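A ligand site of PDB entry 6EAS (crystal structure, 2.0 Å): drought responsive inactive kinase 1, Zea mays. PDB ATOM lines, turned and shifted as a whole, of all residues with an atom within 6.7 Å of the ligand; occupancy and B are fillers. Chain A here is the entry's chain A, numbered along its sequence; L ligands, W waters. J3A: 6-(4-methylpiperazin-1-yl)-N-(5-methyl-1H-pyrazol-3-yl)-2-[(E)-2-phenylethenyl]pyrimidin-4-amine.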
ATOM      1  N   ILE A  48     -28.234  11.808 -14.437  1.00  0.00           N
ATOM      2  CA  ILE A  48     -29.128  10.796 -13.879  1.00  0.00           C
ATOM      3  C   ILE A  48     -29.962  11.429 -12.764  1.00  0.00           C
ATOM      4  O   ILE A  48     -31.106  11.044 -12.556  1.00  0.00           O
ATOM      5  CB  ILE A  48     -28.319   9.595 -13.347  1.00  0.00           C
ATOM      6  CG1 ILE A  48     -27.535   8.898 -14.465  1.00  0.00           C
ATOM      7  CG2 ILE A  48     -29.199   8.621 -12.583  1.00  0.00           C
ATOM      8  CD1 ILE A  48     -26.366   8.079 -13.964  1.00  0.00           C
ATOM      9  N   GLY A  49     -29.359  12.370 -12.035  1.00  0.00           N
ATOM     10  CA  GLY A  49     -29.937  12.912 -10.810  1.00  0.00           C
ATOM     11  C   GLY A  49     -29.042  13.918 -10.101  1.00  0.00           C
ATOM     12  O   GLY A  49     -27.968  14.318 -10.584  1.00  0.00           O
ATOM     13  N   SER A  50     -29.512  14.348  -8.938  1.00  0.00           N
ATOM     14  CA  SER A  50     -28.913  15.421  -8.182  1.00  0.00           C
ATOM     15  C   SER A  50     -29.349  15.268  -6.730  1.00  0.00           C
ATOM     16  O   SER A  50     -30.512  14.974  -6.482  1.00  0.00           O
ATOM     17  CB  SER A  50     -29.331  16.763  -8.751  1.00  0.00           C
ATOM     18  OG  SER A  50     -28.284  17.707  -8.675  1.00  0.00           O
ATOM     19  N   THR A  51     -28.412  15.386  -5.791  1.00  0.00           N
ATOM     20  CA  THR A  51     -28.704  15.149  -4.377  1.00  0.00           C
ATOM     21  C   THR A  51     -28.111  16.280  -3.534  1.00  0.00           C
ATOM     22  O   THR A  51     -27.613  17.271  -4.068  1.00  0.00           O
ATOM     23  CB  THR A  51     -28.180  13.780  -3.922  1.00  0.00           C
ATOM     24  OG1 THR A  51     -26.782  13.884  -3.653  1.00  0.00           O
ATOM     25  CG2 THR A  51     -28.412  12.693  -4.951  1.00  0.00           C
ATOM     26  N   LEU A  56     -25.036  13.583 -10.256  1.00  0.00           N
ATOM     27  CA  LEU A  56     -24.827  12.251 -10.826  1.00  0.00           C
ATOM     28  C   LEU A  56     -24.919  12.326 -12.355  1.00  0.00           C
ATOM     29  O   LEU A  56     -25.947  12.741 -12.873  1.00  0.00           O
ATOM     30  CB  LEU A  56     -25.885  11.287 -10.287  1.00  0.00           C
ATOM     31  CG  LEU A  56     -25.843  11.044  -8.779  1.00  0.00           C
ATOM     32  CD1 LEU A  56     -27.009  10.179  -8.331  1.00  0.00           C
ATOM     33  CD2 LEU A  56     -24.520  10.393  -8.362  1.00  0.00           C
ATOM     34  N   ILE A  67     -21.434   3.399 -15.933  1.00  0.00           N
ATOM     35  CA  ILE A  67     -21.008   4.060 -14.706  1.00  0.00           C
ATOM     36  C   ILE A  67     -21.999   5.172 -14.368  1.00  0.00           C
ATOM     37  O   ILE A  67     -22.657   5.737 -15.241  1.00  0.00           O
ATOM     38  CB  ILE A  67     -19.566   4.606 -14.802  1.00  0.00           C
ATOM     39  CG1 ILE A  67     -19.406   5.677 -15.887  1.00  0.00           C
ATOM     40  CG2 ILE A  67     -18.557   3.475 -14.953  1.00  0.00           C
ATOM     41  CD1 ILE A  67     -18.089   6.411 -15.828  1.00  0.00           C
ATOM     42  N   ALA A  68     -22.075   5.457 -13.056  1.00  0.00           N
ATOM     43  CA  ALA A  68     -22.735   6.600 -12.469  1.00  0.00           C
ATOM     44  C   ALA A  68     -21.670   7.455 -11.773  1.00  0.00           C
ATOM     45  O   ALA A  68     -21.029   6.996 -10.812  1.00  0.00           O
ATOM     46  CB  ALA A  68     -23.799   6.125 -11.497  1.00  0.00           C
ATOM     47  N   VAL A  69     -21.439   8.664 -12.271  1.00  0.00           N
ATOM     48  CA  VAL A  69     -20.397   9.517 -11.773  1.00  0.00           C
ATOM     49  C   VAL A  69     -20.992  10.515 -10.790  1.00  0.00           C
ATOM     50  O   VAL A  69     -21.848  11.319 -11.152  1.00  0.00           O
ATOM     51  CB  VAL A  69     -19.662  10.204 -12.931  1.00  0.00           C
ATOM     52  CG1 VAL A  69     -18.666  11.239 -12.432  1.00  0.00           C
ATOM     53  CG2 VAL A  69     -18.998   9.192 -13.845  1.00  0.00           C
ATOM     54  N   ALA A  70     -20.520  10.477  -9.540  1.00  0.00           N
ATOM     55  CA  ALA A  70     -20.952  11.422  -8.501  1.00  0.00           C
ATOM     56  C   ALA A  70     -19.918  12.540  -8.358  1.00  0.00           C
ATOM     57  O   ALA A  70     -18.793  12.289  -7.954  1.00  0.00           O
ATOM     58  CB  ALA A  70     -21.167  10.679  -7.199  1.00  0.00           C
ATOM     59  N   MET A 104     -23.551  -0.913  -4.095  1.00  0.00           N
ATOM     60  CA  MET A 104     -23.232  -0.117  -5.254  1.00  0.00           C
ATOM     61  C   MET A 104     -21.761   0.303  -5.124  1.00  0.00           C
ATOM     62  O   MET A 104     -21.415   1.311  -4.492  1.00  0.00           O
ATOM     63  CB  MET A 104     -24.144   1.106  -5.376  1.00  0.00           C
ATOM     64  CG  MET A 104     -23.792   1.983  -6.559  1.00  0.00           C
ATOM     65  SD  MET A 104     -25.111   3.126  -7.001  1.00  0.00           S
ATOM     66  CE  MET A 104     -26.167   1.953  -7.862  1.00  0.00           C
ATOM     67  N   PHE A 122     -19.277   5.153  -9.618  1.00  0.00           N
ATOM     68  CA  PHE A 122     -19.998   4.020  -9.076  1.00  0.00           C
ATOM     69  C   PHE A 122     -20.537   3.136 -10.200  1.00  0.00           C
ATOM     70  O   PHE A 122     -20.616   3.552 -11.341  1.00  0.00           O
ATOM     71  CB  PHE A 122     -21.145   4.502  -8.199  1.00  0.00           C
ATOM     72  CG  PHE A 122     -20.717   5.140  -6.906  1.00  0.00           C
ATOM     73  CD1 PHE A 122     -20.325   4.361  -5.820  1.00  0.00           C
ATOM     74  CD2 PHE A 122     -20.738   6.516  -6.754  1.00  0.00           C
ATOM     75  CE1 PHE A 122     -19.954   4.962  -4.620  1.00  0.00           C
ATOM     76  CE2 PHE A 122     -20.360   7.110  -5.552  1.00  0.00           C
ATOM     77  CZ  PHE A 122     -19.961   6.329  -4.502  1.00  0.00           C
ATOM     78  N   GLU A 123     -20.862   1.900  -9.838  1.00  0.00           N
ATOM     79  CA  GLU A 123     -21.578   0.961 -10.678  1.00  0.00           C
ATOM     80  C   GLU A 123     -22.873   1.614 -11.136  1.00  0.00           C
ATOM     81  O   GLU A 123     -23.429   2.462 -10.441  1.00  0.00           O
ATOM     82  CB  GLU A 123     -21.871  -0.294  -9.858  1.00  0.00           C
ATOM     83  CG  GLU A 123     -20.651  -1.115  -9.551  1.00  0.00           C
ATOM     84  CD  GLU A 123     -20.957  -2.363  -8.766  1.00  0.00           C
ATOM     85  OE1 GLU A 123     -21.748  -2.270  -7.817  1.00  0.00           O
ATOM     86  OE2 GLU A 123     -20.418  -3.412  -9.085  1.00  0.00           O
ATOM     87  N   TYR A 124     -23.312   1.270 -12.343  1.00  0.00           N
ATOM     88  CA  TYR A 124     -24.562   1.800 -12.843  1.00  0.00           C
ATOM     89  C   TYR A 124     -25.631   0.725 -12.690  1.00  0.00           C
ATOM     90  O   TYR A 124     -25.447  -0.408 -13.159  1.00  0.00           O
ATOM     91  CB  TYR A 124     -24.484   2.227 -14.310  1.00  0.00           C
ATOM     92  CG  TYR A 124     -25.818   2.683 -14.833  1.00  0.00           C
ATOM     93  CD1 TYR A 124     -26.376   3.874 -14.385  1.00  0.00           C
ATOM     94  CD2 TYR A 124     -26.561   1.907 -15.712  1.00  0.00           C
ATOM     95  CE1 TYR A 124     -27.617   4.291 -14.809  1.00  0.00           C
ATOM     96  CE2 TYR A 124     -27.794   2.335 -16.177  1.00  0.00           C
ATOM     97  CZ  TYR A 124     -28.322   3.527 -15.726  1.00  0.00           C
ATOM     98  OH  TYR A 124     -29.552   3.946 -16.130  1.00  0.00           O
ATOM     99  N   ALA A 125     -26.734   1.083 -12.014  1.00  0.00           N
ATOM    100  CA  ALA A 125     -27.886   0.190 -11.829  1.00  0.00           C
ATOM    101  C   ALA A 125     -28.967   0.583 -12.825  1.00  0.00           C
ATOM    102  O   ALA A 125     -29.626   1.601 -12.667  1.00  0.00           O
ATOM    103  CB  ALA A 125     -28.390   0.262 -10.403  1.00  0.00           C
ATOM    104  N   PRO A 126     -29.223  -0.208 -13.879  1.00  0.00           N
ATOM    105  CA  PRO A 126     -30.162   0.217 -14.901  1.00  0.00           C
ATOM    106  C   PRO A 126     -31.638   0.311 -14.452  1.00  0.00           C
ATOM    107  O   PRO A 126     -32.381   1.101 -15.016  1.00  0.00           O
ATOM    108  CB  PRO A 126     -29.920  -0.782 -16.040  1.00  0.00           C
ATOM    109  CG  PRO A 126     -29.402  -2.009 -15.346  1.00  0.00           C
ATOM    110  CD  PRO A 126     -28.590  -1.497 -14.172  1.00  0.00           C
ATOM    111  N   ASN A 127     -32.050  -0.420 -13.405  1.00  0.00           N
ATOM    112  CA  ASN A 127     -33.483  -0.403 -13.030  1.00  0.00           C
ATOM    113  C   ASN A 127     -33.774   0.615 -11.900  1.00  0.00           C
ATOM    114  O   ASN A 127     -34.844   0.566 -11.282  1.00  0.00           O
ATOM    115  CB  ASN A 127     -33.983  -1.811 -12.735  1.00  0.00           C
ATOM    116  CG  ASN A 127     -34.271  -2.556 -14.032  1.00  0.00           C
ATOM    117  OD1 ASN A 127     -35.084  -2.093 -14.830  1.00  0.00           O
ATOM    118  ND2 ASN A 127     -33.642  -3.686 -14.242  1.00  0.00           N
ATOM    119  N   GLY A 128     -32.858   1.560 -11.668  1.00  0.00           N
ATOM    120  CA  GLY A 128     -33.100   2.656 -10.747  1.00  0.00           C
ATOM    121  C   GLY A 128     -33.426   2.188  -9.338  1.00  0.00           C
ATOM    122  O   GLY A 128     -32.976   1.122  -8.911  1.00  0.00           O
ATOM    123  N   THR A 129     -34.219   2.986  -8.608  1.00  0.00           N
ATOM    124  CA  THR A 129     -34.409   2.797  -7.174  1.00  0.00           C
ATOM    125  C   THR A 129     -35.553   1.819  -6.858  1.00  0.00           C
ATOM    126  O   THR A 129     -36.516   1.683  -7.611  1.00  0.00           O
ATOM    127  CB  THR A 129     -34.689   4.106  -6.428  1.00  0.00           C
ATOM    128  OG1 THR A 129     -35.963   4.596  -6.834  1.00  0.00           O
ATOM    129  CG2 THR A 129     -33.598   5.139  -6.667  1.00  0.00           C
ATOM    130  N   GLU A 132     -38.849   3.685  -6.596  1.00  0.00           N
ATOM    131  CA  GLU A 132     -39.538   3.858  -7.883  1.00  0.00           C
ATOM    132  C   GLU A 132     -40.399   2.631  -8.207  1.00  0.00           C
ATOM    133  O   GLU A 132     -41.563   2.788  -8.612  1.00  0.00           O
ATOM    134  CB  GLU A 132     -38.538   4.083  -9.026  1.00  0.00           C
ATOM    135  CG  GLU A 132     -39.208   4.546 -10.300  1.00  0.00           C
ATOM    136  CD  GLU A 132     -38.377   4.411 -11.557  1.00  0.00           C
ATOM    137  OE1 GLU A 132     -37.131   4.311 -11.449  1.00  0.00           O
ATOM    138  OE2 GLU A 132     -38.970   4.400 -12.652  1.00  0.00           O
ATOM    139  N   THR A 176     -35.059   4.847  -1.321  1.00  0.00           N
ATOM    140  CA  THR A 176     -34.561   5.715  -2.375  1.00  0.00           C
ATOM    141  C   THR A 176     -33.043   5.538  -2.544  1.00  0.00           C
ATOM    142  O   THR A 176     -32.486   6.082  -3.487  1.00  0.00           O
ATOM    143  CB  THR A 176     -34.869   7.201  -2.153  1.00  0.00           C
ATOM    144  OG1 THR A 176     -34.033   7.662  -1.096  1.00  0.00           O
ATOM    145  CG2 THR A 176     -36.332   7.456  -1.842  1.00  0.00           C
ATOM    146  N   TYR A 179     -30.743   0.425  -5.057  1.00  0.00           N
ATOM    147  CA  TYR A 179     -30.857   0.394  -6.483  1.00  0.00           C
ATOM    148  C   TYR A 179     -31.045  -1.041  -6.954  1.00  0.00           C
ATOM    149  O   TYR A 179     -30.798  -1.993  -6.206  1.00  0.00           O
ATOM    150  CB  TYR A 179     -29.656   1.081  -7.148  1.00  0.00           C
ATOM    151  CG  TYR A 179     -29.670   2.579  -6.989  1.00  0.00           C
ATOM    152  CD1 TYR A 179     -29.236   3.173  -5.835  1.00  0.00           C
ATOM    153  CD2 TYR A 179     -30.167   3.390  -7.998  1.00  0.00           C
ATOM    154  CE1 TYR A 179     -29.269   4.554  -5.672  1.00  0.00           C
ATOM    155  CE2 TYR A 179     -30.193   4.770  -7.870  1.00  0.00           C
ATOM    156  CZ  TYR A 179     -29.734   5.351  -6.692  1.00  0.00           C
ATOM    157  OH  TYR A 179     -29.797   6.712  -6.558  1.00  0.00           O
ATOM    158  N   LEU A 180     -31.485  -1.184  -8.203  1.00  0.00           N
ATOM    159  CA  LEU A 180     -31.797  -2.479  -8.759  1.00  0.00           C
ATOM    160  C   LEU A 180     -31.026  -2.699 -10.062  1.00  0.00           C
ATOM    161  O   LEU A 180     -31.060  -1.865 -10.963  1.00  0.00           O
ATOM    162  CB  LEU A 180     -33.303  -2.553  -9.005  1.00  0.00           C
ATOM    163  CG  LEU A 180     -34.153  -2.451  -7.751  1.00  0.00           C
ATOM    164  CD1 LEU A 180     -35.584  -2.113  -8.102  1.00  0.00           C
ATOM    165  CD2 LEU A 180     -34.062  -3.736  -6.950  1.00  0.00           C
ATOM    166  N   SER A 189     -26.628   1.732  -1.671  1.00  0.00           N
ATOM    167  CA  SER A 189     -25.696   2.776  -2.083  1.00  0.00           C
ATOM    168  C   SER A 189     -25.278   3.670  -0.912  1.00  0.00           C
ATOM    169  O   SER A 189     -26.002   3.828   0.092  1.00  0.00           O
ATOM    170  CB  SER A 189     -26.317   3.631  -3.118  1.00  0.00           C
ATOM    171  OG  SER A 189     -27.324   4.426  -2.529  1.00  0.00           O
ATOM    172  N   LEU A 191     -23.955   7.355  -1.855  1.00  0.00           N
ATOM    173  CA  LEU A 191     -23.559   8.303  -2.878  1.00  0.00           C
ATOM    174  C   LEU A 191     -23.100   9.632  -2.248  1.00  0.00           C
ATOM    175  O   LEU A 191     -22.221  10.292  -2.801  1.00  0.00           O
ATOM    176  CB  LEU A 191     -24.729   8.524  -3.826  1.00  0.00           C
ATOM    177  CG  LEU A 191     -25.310   7.252  -4.443  1.00  0.00           C
ATOM    178  CD1 LEU A 191     -26.588   7.572  -5.209  1.00  0.00           C
ATOM    179  CD2 LEU A 191     -24.289   6.585  -5.348  1.00  0.00           C
ATOM    180  N   GLU A 192     -23.698  10.002  -1.116  1.00  0.00           N
ATOM    181  CA  GLU A 192     -23.538  11.325  -0.538  1.00  0.00           C
ATOM    182  C   GLU A 192     -22.115  11.517  -0.023  1.00  0.00           C
ATOM    183  O   GLU A 192     -21.601  10.675   0.700  1.00  0.00           O
ATOM    184  CB  GLU A 192     -24.516  11.547   0.619  1.00  0.00           C
ATOM    185  CG  GLU A 192     -25.974  11.520   0.214  1.00  0.00           C
ATOM    186  CD  GLU A 192     -26.300  12.386  -0.998  1.00  0.00           C
ATOM    187  OE1 GLU A 192     -25.977  13.598  -0.961  1.00  0.00           O
ATOM    188  OE2 GLU A 192     -26.850  11.840  -1.978  1.00  0.00           O
HETATM  189  C4  J3A L   1     -30.531   9.851  -7.522  1.00  0.00           C
HETATM  190  C14 J3A L   1     -33.535   4.541 -16.198  1.00  0.00           C
HETATM  191  C5  J3A L   1     -30.795  10.950  -6.723  1.00  0.00           C
HETATM  192  C6  J3A L   1     -31.630  11.952  -7.164  1.00  0.00           C
HETATM  193  C11 J3A L   1     -31.099   4.593 -12.770  1.00  0.00           C
HETATM  194  C7  J3A L   1     -30.824   8.562  -9.633  1.00  0.00           C
HETATM  195  C8  J3A L   1     -31.685   7.973 -10.439  1.00  0.00           C
HETATM  196  C9  J3A L   1     -31.442   6.766 -11.249  1.00  0.00           C
HETATM  197  C10 J3A L   1     -32.236   5.392 -12.927  1.00  0.00           C
HETATM  198  C12 J3A L   1     -30.146   4.970 -11.814  1.00  0.00           C
HETATM  199  C13 J3A L   1     -33.171   4.054 -14.806  1.00  0.00           C
HETATM  200  N1  J3A L   1     -32.396   6.487 -12.150  1.00  0.00           N
HETATM  201  N2  J3A L   1     -30.340   6.030 -11.046  1.00  0.00           N
HETATM  202  C3  J3A L   1     -31.094   9.738  -8.791  1.00  0.00           C
HETATM  203  N3  J3A L   1     -33.239   5.111 -13.816  1.00  0.00           N
HETATM  204  C1  J3A L   1     -32.203  11.862  -8.419  1.00  0.00           C
HETATM  205  C2  J3A L   1     -31.948  10.753  -9.222  1.00  0.00           C
HETATM  206  N4  J3A L   1     -33.969   5.938 -16.176  1.00  0.00           N
HETATM  207  C15 J3A L   1     -35.027   6.096 -15.185  1.00  0.00           C
HETATM  208  C16 J3A L   1     -34.519   5.807 -13.787  1.00  0.00           C
HETATM  209  C17 J3A L   1     -34.419   6.372 -17.500  1.00  0.00           C
HETATM  210  N5  J3A L   1     -29.002   4.197 -11.637  1.00  0.00           N
HETATM  211  C18 J3A L   1     -27.867   4.469 -10.888  1.00  0.00           C
HETATM  212  N6  J3A L   1     -26.805   3.683 -10.948  1.00  0.00           N
HETATM  213  N7  J3A L   1     -25.915   4.217 -10.076  1.00  0.00           N
HETATM  214  C19 J3A L   1     -26.392   5.311  -9.486  1.00  0.00           C
HETATM  215  C20 J3A L   1     -27.667   5.499  -9.960  1.00  0.00           C
HETATM  216  C21 J3A L   1     -25.586   6.080  -8.493  1.00  0.00           C
HETATM  217  O   HOH W   1     -36.554   3.214 -13.927  1.00  0.00           O
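The backbone carbonyl oxygen (O) of Glu 123 lies within hydrogen-bond range of a nitrogen (N7) of the ligand, 3.1 Å away.
The side-chain sulfur of Met 104 lies close to a nitrogen (N7) of the ligand (3.4 Å).
O of Ala 125 is in hydrogen-bond range of N5 of the ligand (2.9 Å).
N6 of the ligand lies within hydrogen-bond range of N of Ala 125 (2.8 Å).
The backbone carbonyl oxygen (O) of Gly 128 is in hydrogen-bond range of the backbone NH (N) of Leu 180 (2.8 Å).
The backbone NH of Glu 132 is in hydrogen-bond range of the side-chain hydroxyl of Thr 129, at 3.0 Å.
N of Ile 48 sits at hydrogen-bond distance from O of Leu 56 (2.9 Å).
The backbone NH (N) of Leu 56 sits at hydrogen-bond distance from the backbone carbonyl oxygen (O) of Gly 49, at 3.0 Å.
The side-chain hydroxyl of Thr 51 is in hydrogen-bond range of the side-chain carboxylate of Glu 192.
O of Ala 68 is in hydrogen-bond range of N of Phe 122 (2.8 Å).
Merely in contact with the ligand: Pro 126, Ala 68, Ile 48, Ser 50, Gly 49, Tyr 179, Leu 191, Gly 128, Thr 51, Tyr 124, Leu 56 and Glu 132.
Hydrophobic or aromatic side chains that line the ligand: Ile 48, Leu 56, Ala 68, Met 104, Tyr 124, Ala 125, Tyr 179 and Leu 191.
15 residues have an atom within 4 Å of the ligand: Ile 48, Gly 49, Ser 50, Thr 51, Leu 56, Ala 68, Met 104, Glu 123, Tyr 124, Ala 125, Pro 126, Gly 128, Glu 132, Tyr 179 and Leu 191.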
